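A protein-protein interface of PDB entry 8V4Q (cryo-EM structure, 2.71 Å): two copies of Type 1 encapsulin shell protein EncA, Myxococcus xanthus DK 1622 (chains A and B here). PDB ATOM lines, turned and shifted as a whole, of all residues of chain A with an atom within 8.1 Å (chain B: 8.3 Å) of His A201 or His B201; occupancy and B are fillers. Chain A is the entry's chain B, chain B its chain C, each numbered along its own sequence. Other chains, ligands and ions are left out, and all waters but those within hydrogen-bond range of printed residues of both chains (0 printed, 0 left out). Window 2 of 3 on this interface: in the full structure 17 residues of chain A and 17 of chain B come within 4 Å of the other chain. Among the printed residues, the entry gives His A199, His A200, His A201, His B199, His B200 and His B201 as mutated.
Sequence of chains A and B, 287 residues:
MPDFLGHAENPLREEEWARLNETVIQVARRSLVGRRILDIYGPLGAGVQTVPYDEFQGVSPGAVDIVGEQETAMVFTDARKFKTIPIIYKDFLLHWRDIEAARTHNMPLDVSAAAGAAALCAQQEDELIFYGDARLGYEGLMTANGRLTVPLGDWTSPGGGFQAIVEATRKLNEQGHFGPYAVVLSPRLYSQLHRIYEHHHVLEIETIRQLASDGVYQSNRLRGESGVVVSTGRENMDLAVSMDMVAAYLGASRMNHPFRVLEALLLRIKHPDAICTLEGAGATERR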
ATOM      1  N   ILE A 196       4.848  -3.941   2.089  1.00  0.00           N
ATOM      2  CA  ILE A 196       6.265  -3.681   2.314  1.00  0.00           C
ATOM      3  C   ILE A 196       6.901  -4.922   2.930  1.00  0.00           C
ATOM      4  O   ILE A 196       6.368  -5.485   3.892  1.00  0.00           O
ATOM      5  CB  ILE A 196       6.479  -2.454   3.220  1.00  0.00           C
ATOM      6  CG1 ILE A 196       6.001  -1.182   2.517  1.00  0.00           C
ATOM      7  CG2 ILE A 196       7.940  -2.324   3.618  1.00  0.00           C
ATOM      8  CD1 ILE A 196       5.943   0.029   3.421  1.00  0.00           C
ATOM      9  N   TYR A 197       8.034  -5.342   2.373  1.00  0.00           N
ATOM     10  CA  TYR A 197       8.797  -6.470   2.886  1.00  0.00           C
ATOM     11  C   TYR A 197      10.252  -6.061   3.070  1.00  0.00           C
ATOM     12  O   TYR A 197      10.715  -5.062   2.513  1.00  0.00           O
ATOM     13  CB  TYR A 197       8.710  -7.690   1.955  1.00  0.00           C
ATOM     14  CG  TYR A 197       7.310  -8.025   1.494  1.00  0.00           C
ATOM     15  CD1 TYR A 197       6.769  -7.430   0.362  1.00  0.00           C
ATOM     16  CD2 TYR A 197       6.531  -8.941   2.188  1.00  0.00           C
ATOM     17  CE1 TYR A 197       5.489  -7.736  -0.063  1.00  0.00           C
ATOM     18  CE2 TYR A 197       5.251  -9.253   1.771  1.00  0.00           C
ATOM     19  CZ  TYR A 197       4.736  -8.647   0.645  1.00  0.00           C
ATOM     20  OH  TYR A 197       3.463  -8.955   0.225  1.00  0.00           O
ATOM     21  N   GLU A 198      10.970  -6.848   3.866  1.00  0.00           N
ATOM     22  CA  GLU A 198      12.370  -6.569   4.151  1.00  0.00           C
ATOM     23  C   GLU A 198      13.263  -7.031   3.006  1.00  0.00           C
ATOM     24  O   GLU A 198      12.967  -8.008   2.311  1.00  0.00           O
ATOM     25  CB  GLU A 198      12.797  -7.247   5.455  1.00  0.00           C
ATOM     26  CG  GLU A 198      12.843  -8.768   5.392  1.00  0.00           C
ATOM     27  CD  GLU A 198      11.496  -9.413   5.656  1.00  0.00           C
ATOM     28  OE1 GLU A 198      10.466  -8.707   5.585  1.00  0.00           O
ATOM     29  OE2 GLU A 198      11.464 -10.630   5.935  1.00  0.00           O
ATOM     30  N   HIS A 199      14.358  -6.297   2.801  1.00  0.00           N
ATOM     31  CA  HIS A 199      15.392  -6.540   1.796  1.00  0.00           C
ATOM     32  C   HIS A 199      14.905  -6.329   0.368  1.00  0.00           C
ATOM     33  O   HIS A 199      15.709  -6.445  -0.563  1.00  0.00           O
ATOM     34  CB  HIS A 199      15.994  -7.951   1.889  1.00  0.00           C
ATOM     35  CG  HIS A 199      16.395  -8.355   3.273  1.00  0.00           C
ATOM     36  ND1 HIS A 199      16.060  -9.576   3.816  1.00  0.00           N
ATOM     37  CD2 HIS A 199      17.121  -7.710   4.216  1.00  0.00           C
ATOM     38  CE1 HIS A 199      16.550  -9.662   5.040  1.00  0.00           C
ATOM     39  NE2 HIS A 199      17.201  -8.544   5.305  1.00  0.00           N
ATOM     40  N   HIS A 200      13.626  -6.021   0.157  1.00  0.00           N
ATOM     41  CA  HIS A 200      13.099  -5.919  -1.197  1.00  0.00           C
ATOM     42  C   HIS A 200      13.260  -4.518  -1.773  1.00  0.00           C
ATOM     43  O   HIS A 200      13.610  -4.372  -2.950  1.00  0.00           O
ATOM     44  CB  HIS A 200      11.629  -6.343  -1.218  1.00  0.00           C
ATOM     45  CG  HIS A 200      11.436  -7.827  -1.175  1.00  0.00           C
ATOM     46  ND1 HIS A 200      11.387  -8.604  -2.312  1.00  0.00           N
ATOM     47  CD2 HIS A 200      11.295  -8.678  -0.132  1.00  0.00           C
ATOM     48  CE1 HIS A 200      11.216  -9.870  -1.972  1.00  0.00           C
ATOM     49  NE2 HIS A 200      11.158  -9.941  -0.655  1.00  0.00           N
ATOM     50  N   HIS A 201      13.004  -3.489  -0.969  1.00  0.00           N
ATOM     51  CA  HIS A 201      13.334  -2.099  -1.271  1.00  0.00           C
ATOM     52  C   HIS A 201      12.611  -1.559  -2.502  1.00  0.00           C
ATOM     53  O   HIS A 201      12.994  -0.503  -3.022  1.00  0.00           O
ATOM     54  CB  HIS A 201      14.849  -1.914  -1.438  1.00  0.00           C
ATOM     55  CG  HIS A 201      15.641  -2.253  -0.210  1.00  0.00           C
ATOM     56  ND1 HIS A 201      16.947  -1.849  -0.035  1.00  0.00           N
ATOM     57  CD2 HIS A 201      15.311  -2.953   0.900  1.00  0.00           C
ATOM     58  CE1 HIS A 201      17.388  -2.289   1.131  1.00  0.00           C
ATOM     59  NE2 HIS A 201      16.415  -2.961   1.718  1.00  0.00           N
ATOM     60  N   VAL A 202      11.581  -2.247  -2.987  1.00  0.00           N
ATOM     61  CA  VAL A 202      10.826  -1.780  -4.146  1.00  0.00           C
ATOM     62  C   VAL A 202       9.417  -2.349  -4.053  1.00  0.00           C
ATOM     63  O   VAL A 202       9.220  -3.493  -3.635  1.00  0.00           O
ATOM     64  CB  VAL A 202      11.528  -2.171  -5.469  1.00  0.00           C
ATOM     65  CG1 VAL A 202      11.738  -3.676  -5.549  1.00  0.00           C
ATOM     66  CG2 VAL A 202      10.742  -1.666  -6.673  1.00  0.00           C
ATOM     67  N   LEU A 203       8.435  -1.535  -4.434  1.00  0.00           N
ATOM     68  CA  LEU A 203       7.039  -1.945  -4.426  1.00  0.00           C
ATOM     69  C   LEU A 203       6.676  -2.597  -5.754  1.00  0.00           C
ATOM     70  O   LEU A 203       7.048  -2.103  -6.822  1.00  0.00           O
ATOM     71  CB  LEU A 203       6.127  -0.747  -4.168  1.00  0.00           C
ATOM     72  CG  LEU A 203       6.243  -0.082  -2.795  1.00  0.00           C
ATOM     73  CD1 LEU A 203       5.043   0.810  -2.533  1.00  0.00           C
ATOM     74  CD2 LEU A 203       6.392  -1.125  -1.701  1.00  0.00           C
ATOM     75  N   GLU A 204       5.937  -3.706  -5.680  1.00  0.00           N
ATOM     76  CA  GLU A 204       5.598  -4.455  -6.884  1.00  0.00           C
ATOM     77  C   GLU A 204       4.657  -3.682  -7.802  1.00  0.00           C
ATOM     78  O   GLU A 204       4.601  -3.973  -9.004  1.00  0.00           O
ATOM     79  CB  GLU A 204       4.992  -5.807  -6.493  1.00  0.00           C
ATOM     80  CG  GLU A 204       4.751  -6.764  -7.647  1.00  0.00           C
ATOM     81  CD  GLU A 204       4.271  -8.123  -7.178  1.00  0.00           C
ATOM     82  OE1 GLU A 204       4.102  -8.299  -5.954  1.00  0.00           O
ATOM     83  OE2 GLU A 204       4.060  -9.012  -8.030  1.00  0.00           O
ATOM     84  N   ILE B 196      11.893  -9.311  -8.953  1.00  0.00           N
ATOM     85  CA  ILE B 196      12.205  -8.712  -7.627  1.00  0.00           C
ATOM     86  C   ILE B 196      12.920  -9.764  -6.779  1.00  0.00           C
ATOM     87  O   ILE B 196      12.380 -10.878  -6.629  1.00  0.00           O
ATOM     88  CB  ILE B 196      10.916  -8.202  -6.948  1.00  0.00           C
ATOM     89  CG1 ILE B 196      10.801  -6.677  -7.019  1.00  0.00           C
ATOM     90  CG2 ILE B 196      10.811  -8.704  -5.516  1.00  0.00           C
ATOM     91  CD1 ILE B 196       9.433  -6.148  -6.656  1.00  0.00           C
ATOM     92  N   TYR B 197      14.102  -9.430  -6.278  1.00  0.00           N
ATOM     93  CA  TYR B 197      14.888 -10.318  -5.436  1.00  0.00           C
ATOM     94  C   TYR B 197      15.258  -9.606  -4.143  1.00  0.00           C
ATOM     95  O   TYR B 197      15.168  -8.380  -4.032  1.00  0.00           O
ATOM     96  CB  TYR B 197      16.163 -10.799  -6.142  1.00  0.00           C
ATOM     97  CG  TYR B 197      15.927 -11.590  -7.407  1.00  0.00           C
ATOM     98  CD1 TYR B 197      15.588 -12.936  -7.353  1.00  0.00           C
ATOM     99  CD2 TYR B 197      16.064 -11.000  -8.656  1.00  0.00           C
ATOM    100  CE1 TYR B 197      15.379 -13.668  -8.506  1.00  0.00           C
ATOM    101  CE2 TYR B 197      15.858 -11.723  -9.815  1.00  0.00           C
ATOM    102  CZ  TYR B 197      15.515 -13.057  -9.734  1.00  0.00           C
ATOM    103  OH  TYR B 197      15.308 -13.782 -10.885  1.00  0.00           O
ATOM    104  N   GLU B 198      15.678 -10.395  -3.159  1.00  0.00           N
ATOM    105  CA  GLU B 198      16.077  -9.861  -1.867  1.00  0.00           C
ATOM    106  C   GLU B 198      17.546  -9.458  -1.875  1.00  0.00           C
ATOM    107  O   GLU B 198      18.355  -9.984  -2.646  1.00  0.00           O
ATOM    108  CB  GLU B 198      15.827 -10.889  -0.762  1.00  0.00           C
ATOM    109  CG  GLU B 198      16.717 -12.125  -0.844  1.00  0.00           C
ATOM    110  CD  GLU B 198      16.199 -13.169  -1.818  1.00  0.00           C
ATOM    111  OE1 GLU B 198      15.320 -12.842  -2.643  1.00  0.00           O
ATOM    112  OE2 GLU B 198      16.677 -14.321  -1.760  1.00  0.00           O
ATOM    113  N   HIS B 199      17.879  -8.492  -1.015  1.00  0.00           N
ATOM    114  CA  HIS B 199      19.253  -8.059  -0.772  1.00  0.00           C
ATOM    115  C   HIS B 199      19.904  -7.437  -2.004  1.00  0.00           C
ATOM    116  O   HIS B 199      21.108  -7.159  -1.995  1.00  0.00           O
ATOM    117  CB  HIS B 199      20.104  -9.229  -0.267  1.00  0.00           C
ATOM    118  CG  HIS B 199      19.680  -9.754   1.070  1.00  0.00           C
ATOM    119  ND1 HIS B 199      19.309 -11.065   1.269  1.00  0.00           N
ATOM    120  CD2 HIS B 199      19.567  -9.144   2.273  1.00  0.00           C
ATOM    121  CE1 HIS B 199      18.987 -11.241   2.539  1.00  0.00           C
ATOM    122  NE2 HIS B 199      19.135 -10.090   3.169  1.00  0.00           N
ATOM    123  N   HIS B 200      19.130  -7.219  -3.067  1.00  0.00           N
ATOM    124  CA  HIS B 200      19.684  -6.596  -4.264  1.00  0.00           C
ATOM    125  C   HIS B 200      19.531  -5.080  -4.230  1.00  0.00           C
ATOM    126  O   HIS B 200      20.385  -4.357  -4.757  1.00  0.00           O
ATOM    127  CB  HIS B 200      19.027  -7.183  -5.511  1.00  0.00           C
ATOM    128  CG  HIS B 200      19.562  -8.527  -5.893  1.00  0.00           C
ATOM    129  ND1 HIS B 200      19.097  -9.699  -5.336  1.00  0.00           N
ATOM    130  CD2 HIS B 200      20.524  -8.886  -6.775  1.00  0.00           C
ATOM    131  CE1 HIS B 200      19.750 -10.722  -5.857  1.00  0.00           C
ATOM    132  NE2 HIS B 200      20.621 -10.256  -6.734  1.00  0.00           N
ATOM    133  N   HIS B 201      18.449  -4.589  -3.632  1.00  0.00           N
ATOM    134  CA  HIS B 201      18.222  -3.176  -3.340  1.00  0.00           C
ATOM    135  C   HIS B 201      18.104  -2.312  -4.592  1.00  0.00           C
ATOM    136  O   HIS B 201      18.026  -1.083  -4.480  1.00  0.00           O
ATOM    137  CB  HIS B 201      19.320  -2.606  -2.429  1.00  0.00           C
ATOM    138  CG  HIS B 201      19.620  -3.455  -1.231  1.00  0.00           C
ATOM    139  ND1 HIS B 201      20.753  -3.286  -0.466  1.00  0.00           N
ATOM    140  CD2 HIS B 201      18.934  -4.477  -0.664  1.00  0.00           C
ATOM    141  CE1 HIS B 201      20.754  -4.167   0.518  1.00  0.00           C
ATOM    142  NE2 HIS B 201      19.661  -4.901   0.421  1.00  0.00           N
ATOM    143  N   VAL B 202      18.087  -2.912  -5.778  1.00  0.00           N
ATOM    144  CA  VAL B 202      18.002  -2.148  -7.018  1.00  0.00           C
ATOM    145  C   VAL B 202      17.477  -3.068  -8.112  1.00  0.00           C
ATOM    146  O   VAL B 202      17.790  -4.261  -8.143  1.00  0.00           O
ATOM    147  CB  VAL B 202      19.372  -1.528  -7.390  1.00  0.00           C
ATOM    148  CG1 VAL B 202      20.415  -2.614  -7.620  1.00  0.00           C
ATOM    149  CG2 VAL B 202      19.246  -0.624  -8.611  1.00  0.00           C
ATOM    150  N   LEU B 203      16.662  -2.506  -8.999  1.00  0.00           N
ATOM    151  CA  LEU B 203      16.175  -3.241 -10.156  1.00  0.00           C
ATOM    152  C   LEU B 203      17.257  -3.306 -11.224  1.00  0.00           C
ATOM    153  O   LEU B 203      17.948  -2.319 -11.490  1.00  0.00           O
ATOM    154  CB  LEU B 203      14.913  -2.586 -10.717  1.00  0.00           C
ATOM    155  CG  LEU B 203      13.584  -2.991 -10.073  1.00  0.00           C
ATOM    156  CD1 LEU B 203      12.410  -2.559 -10.937  1.00  0.00           C
ATOM    157  CD2 LEU B 203      13.539  -4.489  -9.817  1.00  0.00           C
ATOM    158  N   GLU B 204      17.405  -4.485 -11.835  1.00  0.00           N
ATOM    159  CA  GLU B 204      18.463  -4.686 -12.821  1.00  0.00           C
ATOM    160  C   GLU B 204      18.282  -3.792 -14.040  1.00  0.00           C
ATOM    161  O   GLU B 204      19.254  -3.509 -14.752  1.00  0.00           O
ATOM    162  CB  GLU B 204      18.507  -6.155 -13.243  1.00  0.00           C
ATOM    163  CG  GLU B 204      19.858  -6.617 -13.758  1.00  0.00           C
ATOM    164  CD  GLU B 204      20.084  -8.099 -13.537  1.00  0.00           C
ATOM    165  OE1 GLU B 204      19.468  -8.664 -12.608  1.00  0.00           O
ATOM    166  OE2 GLU B 204      20.875  -8.702 -14.291  1.00  0.00           O
ATOM    167  N   THR B 207      20.319  -0.747 -13.556  1.00  0.00           N
ATOM    168  CA  THR B 207      21.730  -1.076 -13.718  1.00  0.00           C
ATOM    169  C   THR B 207      22.096  -1.173 -15.195  1.00  0.00           C
ATOM    170  O   THR B 207      23.183  -0.748 -15.603  1.00  0.00           O
ATOM    171  CB  THR B 207      22.045  -2.382 -12.989  1.00  0.00           C
ATOM    172  OG1 THR B 207      21.733  -2.237 -11.598  1.00  0.00           O
ATOM    173  CG2 THR B 207      23.517  -2.725 -13.120  1.00  0.00           C
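The backbone carbonyl oxygen of His A199 is in hydrogen-bond range of the backbone NH of His B199 (3.0 Å).
ND1 of His B200 lies within hydrogen-bond range of O of Glu B198, at 2.8 Å.
Among the printed residues, pairs that only touch across the chains: His A199 with Glu B198 (3.7 Å), His A199 with His B201 (3.8 Å), His A200 with Ile B196 (3.3 Å), His A201 with His B201 (3.2 Å) and Val A202 with Ile B196 (3.5 Å).
His A201 touches just one residue of chain B: His B201.
His B201 touches just these residues of chain A: His A199 (3.8 Å) and His A201 (3.2 Å).
Printed residues of chain B within 4 Å of His A199: Glu B198 (3.7 Å), His B199 (3.0 Å) and His B201 (3.8 Å).
Of the printed residues of chain A, Glu B198 touches His A199 (3.7 Å).
The nearest residue of chain B that does not touch His A201 is Val B202 (5.5 Å).
Along chain B the printed residues that touch a printed residue of chain A span positions 196 to 201.
Of the 9 printed residues of chain A, 4 touch a printed residue of chain B.
Printed residues of chain A that touch a printed residue of chain B: His A199, His A200, His A201 and Val A202.
Hydrophobic or aromatic side chains of chain A that line the printed part of chain B: His A199, His A200, His A201 and Val A202.
Among the printed residues, no Asp or Glu carboxylate lies within 4 Å of a Lys or Arg side-chain nitrogen of the other chain.
His A199 touches Glu B198, but with the chains exchanged Glu A198 does not touch His B199 (6.0 Å).
His A199 touches its own counterpart, His B199.
His A199 touches His B201, but with the chains exchanged His A201 does not touch His B199 (6.3 Å).
His A200 touches Ile B196, but with the chains exchanged Ile A196 does not touch His B200 (13.8 Å).
Positions printed for both chains: 196, 197, 198, 199, 200, 201, 202, 203 and 204.
Of the 6 pairs that touch across the chains among the printed residues, 2 have their exchanged pair printed and touching as well.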
